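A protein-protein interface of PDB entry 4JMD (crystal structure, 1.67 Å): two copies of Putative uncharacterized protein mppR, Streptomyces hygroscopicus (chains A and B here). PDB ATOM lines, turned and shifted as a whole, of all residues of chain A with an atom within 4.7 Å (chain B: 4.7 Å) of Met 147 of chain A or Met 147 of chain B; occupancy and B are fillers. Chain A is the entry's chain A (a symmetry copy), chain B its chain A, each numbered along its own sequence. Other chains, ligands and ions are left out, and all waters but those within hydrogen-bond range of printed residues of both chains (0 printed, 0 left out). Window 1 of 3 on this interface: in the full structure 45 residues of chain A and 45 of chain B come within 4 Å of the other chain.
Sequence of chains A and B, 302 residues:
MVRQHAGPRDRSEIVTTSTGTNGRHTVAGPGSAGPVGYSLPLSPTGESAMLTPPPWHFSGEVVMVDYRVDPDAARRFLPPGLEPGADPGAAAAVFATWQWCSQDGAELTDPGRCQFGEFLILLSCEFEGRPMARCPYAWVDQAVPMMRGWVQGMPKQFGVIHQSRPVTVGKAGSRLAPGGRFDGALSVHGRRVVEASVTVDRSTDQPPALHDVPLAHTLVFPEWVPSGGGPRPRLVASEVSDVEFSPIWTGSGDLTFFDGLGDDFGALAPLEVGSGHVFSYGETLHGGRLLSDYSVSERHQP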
ATOM      1  N   MET A  50      18.579   7.009 -13.915  1.00  0.00           N
ATOM      2  CA  MET A  50      18.346   7.676 -15.194  1.00  0.00           C
ATOM      3  C   MET A  50      18.989   9.079 -15.255  1.00  0.00           C
ATOM      4  O   MET A  50      19.542   9.469 -16.312  1.00  0.00           O
ATOM      5  CB  MET A  50      16.836   7.771 -15.462  1.00  0.00           C
ATOM      6  CG  MET A  50      16.534   8.120 -16.913  1.00  0.00           C
ATOM      7  SD  MET A  50      14.768   8.214 -17.170  1.00  0.00           S
ATOM      8  CE  MET A  50      14.662   9.874 -16.717  1.00  0.00           C
ATOM      9  N   LEU A  51      18.937   9.805 -14.148  1.00  0.00           N
ATOM     10  CA  LEU A  51      19.428  11.179 -14.057  1.00  0.00           C
ATOM     11  C   LEU A  51      20.678  11.230 -13.195  1.00  0.00           C
ATOM     12  O   LEU A  51      20.853  10.412 -12.286  1.00  0.00           O
ATOM     13  CB  LEU A  51      18.354  12.059 -13.452  1.00  0.00           C
ATOM     14  CG  LEU A  51      17.008  12.080 -14.190  1.00  0.00           C
ATOM     15  CD1 LEU A  51      16.085  13.064 -13.491  1.00  0.00           C
ATOM     16  CD2 LEU A  51      17.234  12.488 -15.663  1.00  0.00           C
ATOM     17  N   ALA A 143      13.956  11.523 -23.688  1.00  0.00           N
ATOM     18  CA  ALA A 143      13.380  11.164 -22.387  1.00  0.00           C
ATOM     19  C   ALA A 143      14.115  11.723 -21.171  1.00  0.00           C
ATOM     20  O   ALA A 143      13.476  12.115 -20.179  1.00  0.00           O
ATOM     21  CB  ALA A 143      13.281   9.650 -22.278  1.00  0.00           C
ATOM     22  N   VAL A 144      15.449  11.692 -21.192  1.00  0.00           N
ATOM     23  CA  VAL A 144      16.187  12.175 -20.035  1.00  0.00           C
ATOM     24  C   VAL A 144      15.890  13.662 -19.809  1.00  0.00           C
ATOM     25  O   VAL A 144      15.544  14.060 -18.703  1.00  0.00           O
ATOM     26  CB  VAL A 144      17.705  11.875 -20.120  1.00  0.00           C
ATOM     27  CG1 VAL A 144      18.514  12.759 -19.169  1.00  0.00           C
ATOM     28  CG2 VAL A 144      17.959  10.401 -19.816  1.00  0.00           C
ATOM     29  N   PRO A 145      15.971  14.486 -20.860  1.00  0.00           N
ATOM     30  CA  PRO A 145      15.622  15.886 -20.616  1.00  0.00           C
ATOM     31  C   PRO A 145      14.177  16.053 -20.173  1.00  0.00           C
ATOM     32  O   PRO A 145      13.902  16.944 -19.354  1.00  0.00           O
ATOM     33  CB  PRO A 145      15.887  16.553 -21.968  1.00  0.00           C
ATOM     34  CG  PRO A 145      16.987  15.717 -22.568  1.00  0.00           C
ATOM     35  CD  PRO A 145      16.722  14.299 -22.111  1.00  0.00           C
ATOM     36  N   MET A 146      13.273  15.230 -20.698  1.00  0.00           N
ATOM     37  CA  MET A 146      11.874  15.367 -20.296  1.00  0.00           C
ATOM     38  C   MET A 146      11.704  15.180 -18.784  1.00  0.00           C
ATOM     39  O   MET A 146      11.118  16.022 -18.095  1.00  0.00           O
ATOM     40  CB  MET A 146      10.959  14.418 -21.055  1.00  0.00           C
ATOM     41  CG  MET A 146       9.501  14.627 -20.660  1.00  0.00           C
ATOM     42  SD  MET A 146       8.416  13.548 -21.611  1.00  0.00           S
ATOM     43  CE  MET A 146       9.069  11.954 -21.149  1.00  0.00           C
ATOM     44  N   MET A 147      12.231  14.081 -18.253  1.00  0.00           N
ATOM     45  CA  MET A 147      12.117  13.802 -16.823  1.00  0.00           C
ATOM     46  C   MET A 147      12.842  14.862 -16.015  1.00  0.00           C
ATOM     47  O   MET A 147      12.339  15.340 -15.006  1.00  0.00           O
ATOM     48  CB  MET A 147      12.695  12.424 -16.492  1.00  0.00           C
ATOM     49  CG  MET A 147      12.467  11.973 -15.034  1.00  0.00           C
ATOM     50  SD  MET A 147      10.731  11.691 -14.673  1.00  0.00           S
ATOM     51  CE  MET A 147      10.429  10.203 -15.640  1.00  0.00           C
ATOM     52  N   ARG A 148      14.049  15.199 -16.443  1.00  0.00           N
ATOM     53  CA  ARG A 148      14.841  16.193 -15.721  1.00  0.00           C
ATOM     54  C   ARG A 148      14.103  17.520 -15.668  1.00  0.00           C
ATOM     55  O   ARG A 148      14.243  18.278 -14.714  1.00  0.00           O
ATOM     56  CB  ARG A 148      16.205  16.380 -16.408  1.00  0.00           C
ATOM     57  CG  ARG A 148      17.232  17.077 -15.559  1.00  0.00           C
ATOM     58  CD  ARG A 148      18.633  16.962 -16.152  1.00  0.00           C
ATOM     59  NE  ARG A 148      18.690  17.415 -17.537  1.00  0.00           N
ATOM     60  CZ  ARG A 148      19.507  16.897 -18.452  1.00  0.00           C
ATOM     61  NH1 ARG A 148      20.376  15.944 -18.103  1.00  0.00           N
ATOM     62  NH2 ARG A 148      19.482  17.350 -19.708  1.00  0.00           N
ATOM     63  N   GLY A 149      13.320  17.818 -16.698  1.00  0.00           N
ATOM     64  CA  GLY A 149      12.508  19.025 -16.679  1.00  0.00           C
ATOM     65  C   GLY A 149      11.540  19.012 -15.524  1.00  0.00           C
ATOM     66  O   GLY A 149      11.421  19.990 -14.790  1.00  0.00           O
ATOM     67  N   TRP A 150      10.840  17.894 -15.334  1.00  0.00           N
ATOM     68  CA  TRP A 150       9.906  17.841 -14.218  1.00  0.00           C
ATOM     69  C   TRP A 150      10.607  17.955 -12.859  1.00  0.00           C
ATOM     70  O   TRP A 150      10.023  18.470 -11.890  1.00  0.00           O
ATOM     71  CB  TRP A 150       9.020  16.605 -14.248  1.00  0.00           C
ATOM     72  CG  TRP A 150       7.964  16.654 -15.321  1.00  0.00           C
ATOM     73  CD1 TRP A 150       8.119  17.120 -16.600  1.00  0.00           C
ATOM     74  CD2 TRP A 150       6.608  16.202 -15.224  1.00  0.00           C
ATOM     75  NE1 TRP A 150       6.940  16.987 -17.293  1.00  0.00           N
ATOM     76  CE2 TRP A 150       5.997  16.442 -16.461  1.00  0.00           C
ATOM     77  CE3 TRP A 150       5.849  15.645 -14.198  1.00  0.00           C
ATOM     78  CZ2 TRP A 150       4.672  16.094 -16.725  1.00  0.00           C
ATOM     79  CZ3 TRP A 150       4.526  15.323 -14.456  1.00  0.00           C
ATOM     80  CH2 TRP A 150       3.955  15.551 -15.696  1.00  0.00           C
ATOM     81  N   VAL A 151      11.849  17.490 -12.767  1.00  0.00           N
ATOM     82  CA  VAL A 151      12.622  17.670 -11.545  1.00  0.00           C
ATOM     83  C   VAL A 151      12.713  19.150 -11.169  1.00  0.00           C
ATOM     84  O   VAL A 151      12.677  19.487  -9.998  1.00  0.00           O
ATOM     85  CB  VAL A 151      14.016  17.022 -11.670  1.00  0.00           C
ATOM     86  CG1 VAL A 151      14.953  17.462 -10.528  1.00  0.00           C
ATOM     87  CG2 VAL A 151      13.858  15.504 -11.646  1.00  0.00           C
ATOM     88  N   MET B  50      -0.321  16.684 -18.707  1.00  0.00           N
ATOM     89  CA  MET B  50       0.165  15.515 -19.438  1.00  0.00           C
ATOM     90  C   MET B  50      -0.526  14.208 -18.993  1.00  0.00           C
ATOM     91  O   MET B  50      -0.838  13.343 -19.845  1.00  0.00           O
ATOM     92  CB  MET B  50       1.688  15.396 -19.270  1.00  0.00           C
ATOM     93  CG  MET B  50       2.299  14.434 -20.279  1.00  0.00           C
ATOM     94  SD  MET B  50       4.069  14.335 -20.043  1.00  0.00           S
ATOM     95  CE  MET B  50       3.969  13.081 -18.864  1.00  0.00           C
ATOM     96  N   LEU B  51      -0.777  14.081 -17.698  1.00  0.00           N
ATOM     97  CA  LEU B  51      -1.354  12.878 -17.099  1.00  0.00           C
ATOM     98  C   LEU B  51      -2.772  13.160 -16.630  1.00  0.00           C
ATOM     99  O   LEU B  51      -3.107  14.292 -16.273  1.00  0.00           O
ATOM    100  CB  LEU B  51      -0.506  12.442 -15.925  1.00  0.00           C
ATOM    101  CG  LEU B  51       0.972  12.161 -16.231  1.00  0.00           C
ATOM    102  CD1 LEU B  51       1.647  11.667 -14.963  1.00  0.00           C
ATOM    103  CD2 LEU B  51       1.074  11.106 -17.356  1.00  0.00           C
ATOM    104  N   ALA B 143       6.188   8.442 -23.899  1.00  0.00           N
ATOM    105  CA  ALA B 143       6.464   9.394 -22.818  1.00  0.00           C
ATOM    106  C   ALA B 143       5.434   9.419 -21.690  1.00  0.00           C
ATOM    107  O   ALA B 143       5.799   9.567 -20.513  1.00  0.00           O
ATOM    108  CB  ALA B 143       6.623  10.789 -23.402  1.00  0.00           C
ATOM    109  N   VAL B 144       4.145   9.359 -22.035  1.00  0.00           N
ATOM    110  CA  VAL B 144       3.130   9.423 -20.996  1.00  0.00           C
ATOM    111  C   VAL B 144       3.280   8.228 -20.045  1.00  0.00           C
ATOM    112  O   VAL B 144       3.333   8.408 -18.834  1.00  0.00           O
ATOM    113  CB  VAL B 144       1.695   9.560 -21.562  1.00  0.00           C
ATOM    114  CG1 VAL B 144       0.636   9.171 -20.529  1.00  0.00           C
ATOM    115  CG2 VAL B 144       1.463  10.991 -22.042  1.00  0.00           C
ATOM    116  N   PRO B 145       3.398   7.009 -20.582  1.00  0.00           N
ATOM    117  CA  PRO B 145       3.599   5.904 -19.645  1.00  0.00           C
ATOM    118  C   PRO B 145       4.888   6.045 -18.851  1.00  0.00           C
ATOM    119  O   PRO B 145       4.911   5.651 -17.674  1.00  0.00           O
ATOM    120  CB  PRO B 145       3.618   4.673 -20.555  1.00  0.00           C
ATOM    121  CG  PRO B 145       2.740   5.071 -21.712  1.00  0.00           C
ATOM    122  CD  PRO B 145       2.973   6.553 -21.915  1.00  0.00           C
ATOM    123  N   MET B 146       5.936   6.583 -19.468  1.00  0.00           N
ATOM    124  CA  MET B 146       7.191   6.729 -18.735  1.00  0.00           C
ATOM    125  C   MET B 146       7.013   7.604 -17.487  1.00  0.00           C
ATOM    126  O   MET B 146       7.373   7.211 -16.372  1.00  0.00           O
ATOM    127  CB  MET B 146       8.312   7.271 -19.609  1.00  0.00           C
ATOM    128  CG  MET B 146       9.622   7.354 -18.834  1.00  0.00           C
ATOM    129  SD  MET B 146      10.961   7.932 -19.892  1.00  0.00           S
ATOM    130  CE  MET B 146      10.312   9.518 -20.385  1.00  0.00           C
ATOM    131  N   MET B 147       6.442   8.791 -17.665  1.00  0.00           N
ATOM    132  CA  MET B 147       6.234   9.705 -16.544  1.00  0.00           C
ATOM    133  C   MET B 147       5.280   9.099 -15.532  1.00  0.00           C
ATOM    134  O   MET B 147       5.505   9.170 -14.331  1.00  0.00           O
ATOM    135  CB  MET B 147       5.676  11.044 -17.033  1.00  0.00           C
ATOM    136  CG  MET B 147       5.584  12.130 -15.941  1.00  0.00           C
ATOM    137  SD  MET B 147       7.200  12.648 -15.357  1.00  0.00           S
ATOM    138  CE  MET B 147       7.805  13.535 -16.800  1.00  0.00           C
ATOM    139  N   ARG B 148       4.190   8.531 -16.025  1.00  0.00           N
ATOM    140  CA  ARG B 148       3.194   7.940 -15.133  1.00  0.00           C
ATOM    141  C   ARG B 148       3.821   6.833 -14.302  1.00  0.00           C
ATOM    142  O   ARG B 148       3.418   6.595 -13.168  1.00  0.00           O
ATOM    143  CB  ARG B 148       2.020   7.377 -15.953  1.00  0.00           C
ATOM    144  CG  ARG B 148       0.784   7.093 -15.144  1.00  0.00           C
ATOM    145  CD  ARG B 148      -0.430   6.839 -16.033  1.00  0.00           C
ATOM    146  NE  ARG B 148      -0.189   5.795 -17.021  1.00  0.00           N
ATOM    147  CZ  ARG B 148      -0.737   5.783 -18.234  1.00  0.00           C
ATOM    148  NH1 ARG B 148      -1.606   6.737 -18.580  1.00  0.00           N
ATOM    149  NH2 ARG B 148      -0.445   4.803 -19.094  1.00  0.00           N
ATOM    150  N   GLY B 149       4.804   6.139 -14.862  1.00  0.00           N
ATOM    151  CA  GLY B 149       5.517   5.127 -14.098  1.00  0.00           C
ATOM    152  C   GLY B 149       6.188   5.729 -12.890  1.00  0.00           C
ATOM    153  O   GLY B 149       6.075   5.209 -11.782  1.00  0.00           O
ATOM    154  N   TRP B 150       6.888   6.847 -13.081  1.00  0.00           N
ATOM    155  CA  TRP B 150       7.536   7.465 -11.931  1.00  0.00           C
ATOM    156  C   TRP B 150       6.531   7.950 -10.880  1.00  0.00           C
ATOM    157  O   TRP B 150       6.842   7.976  -9.676  1.00  0.00           O
ATOM    158  CB  TRP B 150       8.475   8.595 -12.322  1.00  0.00           C
ATOM    159  CG  TRP B 150       9.748   8.117 -12.970  1.00  0.00           C
ATOM    160  CD1 TRP B 150       9.869   7.105 -13.884  1.00  0.00           C
ATOM    161  CD2 TRP B 150      11.068   8.641 -12.778  1.00  0.00           C
ATOM    162  NE1 TRP B 150      11.183   6.972 -14.263  1.00  0.00           N
ATOM    163  CE2 TRP B 150      11.935   7.893 -13.583  1.00  0.00           C
ATOM    164  CE3 TRP B 150      11.597   9.652 -11.981  1.00  0.00           C
ATOM    165  CZ2 TRP B 150      13.304   8.156 -13.659  1.00  0.00           C
ATOM    166  CZ3 TRP B 150      12.960   9.895 -12.041  1.00  0.00           C
ATOM    167  CH2 TRP B 150      13.791   9.154 -12.863  1.00  0.00           C
ATOM    168  N   VAL B 151       5.332   8.332 -11.307  1.00  0.00           N
ATOM    169  CA  VAL B 151       4.286   8.692 -10.360  1.00  0.00           C
ATOM    170  C   VAL B 151       4.023   7.551  -9.376  1.00  0.00           C
ATOM    171  O   VAL B 151       3.764   7.796  -8.209  1.00  0.00           O
ATOM    172  CB  VAL B 151       2.999   9.127 -11.092  1.00  0.00           C
ATOM    173  CG1 VAL B 151       1.797   9.211 -10.131  1.00  0.00           C
ATOM    174  CG2 VAL B 151       3.235  10.490 -11.736  1.00  0.00           C
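The side-chain sulfur of Met 147 of chain B lies close to the side-chain sulfur of Met 147 of chain A (3.7 Å).
Met 50 of chain A touches Trp 150 of chain B. Ala 143 of chain A touches Met 146 of chain B (CB to CE, 3.5 Å). CE of Met 146 of chain A touches CB of Ala 143 of chain B (3.5 Å). CE of Met 146 of chain A touches CE of Met 146 of chain B (2.8 Å). Met 147 of chain A touches Trp 150 of chain B. CZ2 of Trp 150 of chain A touches CE of Met 50 of chain B, at 3.8 Å. CE of Met 147 of chain B touches CD2 of Trp 150 of chain A (3.3 Å).
Printed residues of chain B within 4 Å of Ala 143 of chain A: Met 146. Of the printed residues of chain B, Met 146 of chain A touches Ala 143 and Met 146. Printed residues of chain B within 4 Å of Met 147 of chain A: Met 147 (3.7 Å) and Trp 150 (3.3 Å). Printed residues of chain A within 4 Å of Ala 143 of chain B: Met 146. Of the printed residues of chain A, Met 147 of chain B touches Met 147 and Trp 150.
Of the 11 printed residues of chain B, 5 touch a printed residue of chain A. Hydrophobic or aromatic side chains of chain B that line the printed part of chain A: Met 50, Ala 143, Met 146, Met 147 and Trp 150. Hydrophobic or aromatic side chains of chain A within 4 Å of the printed part of chain B: Met 50, Ala 143, Met 146, Met 147 and Trp 150. Among the printed residues, 8 pairs touch across the chains.
Met 50 of chain A touches Trp 150 of chain B, and with the chains exchanged Trp 150 of chain A touches Met 50 of chain B. Ala 143 of chain A touches Met 146 of chain B, and with the chains exchanged Met 146 of chain A touches Ala 143 of chain B. Met 147 of chain B touches its own counterpart, Met 147 of chain A. Met 147 of chain A touches Trp 150 of chain B, and with the chains exchanged Trp 150 of chain A touches Met 147 of chain B. Positions printed for both chains: 50, 51, 143, 144, 145, 146, 147, 148, 149, 150 and 151. Of the 8 pairs that touch across the chains among the printed residues, 8 have their exchanged pair printed and touching as well.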
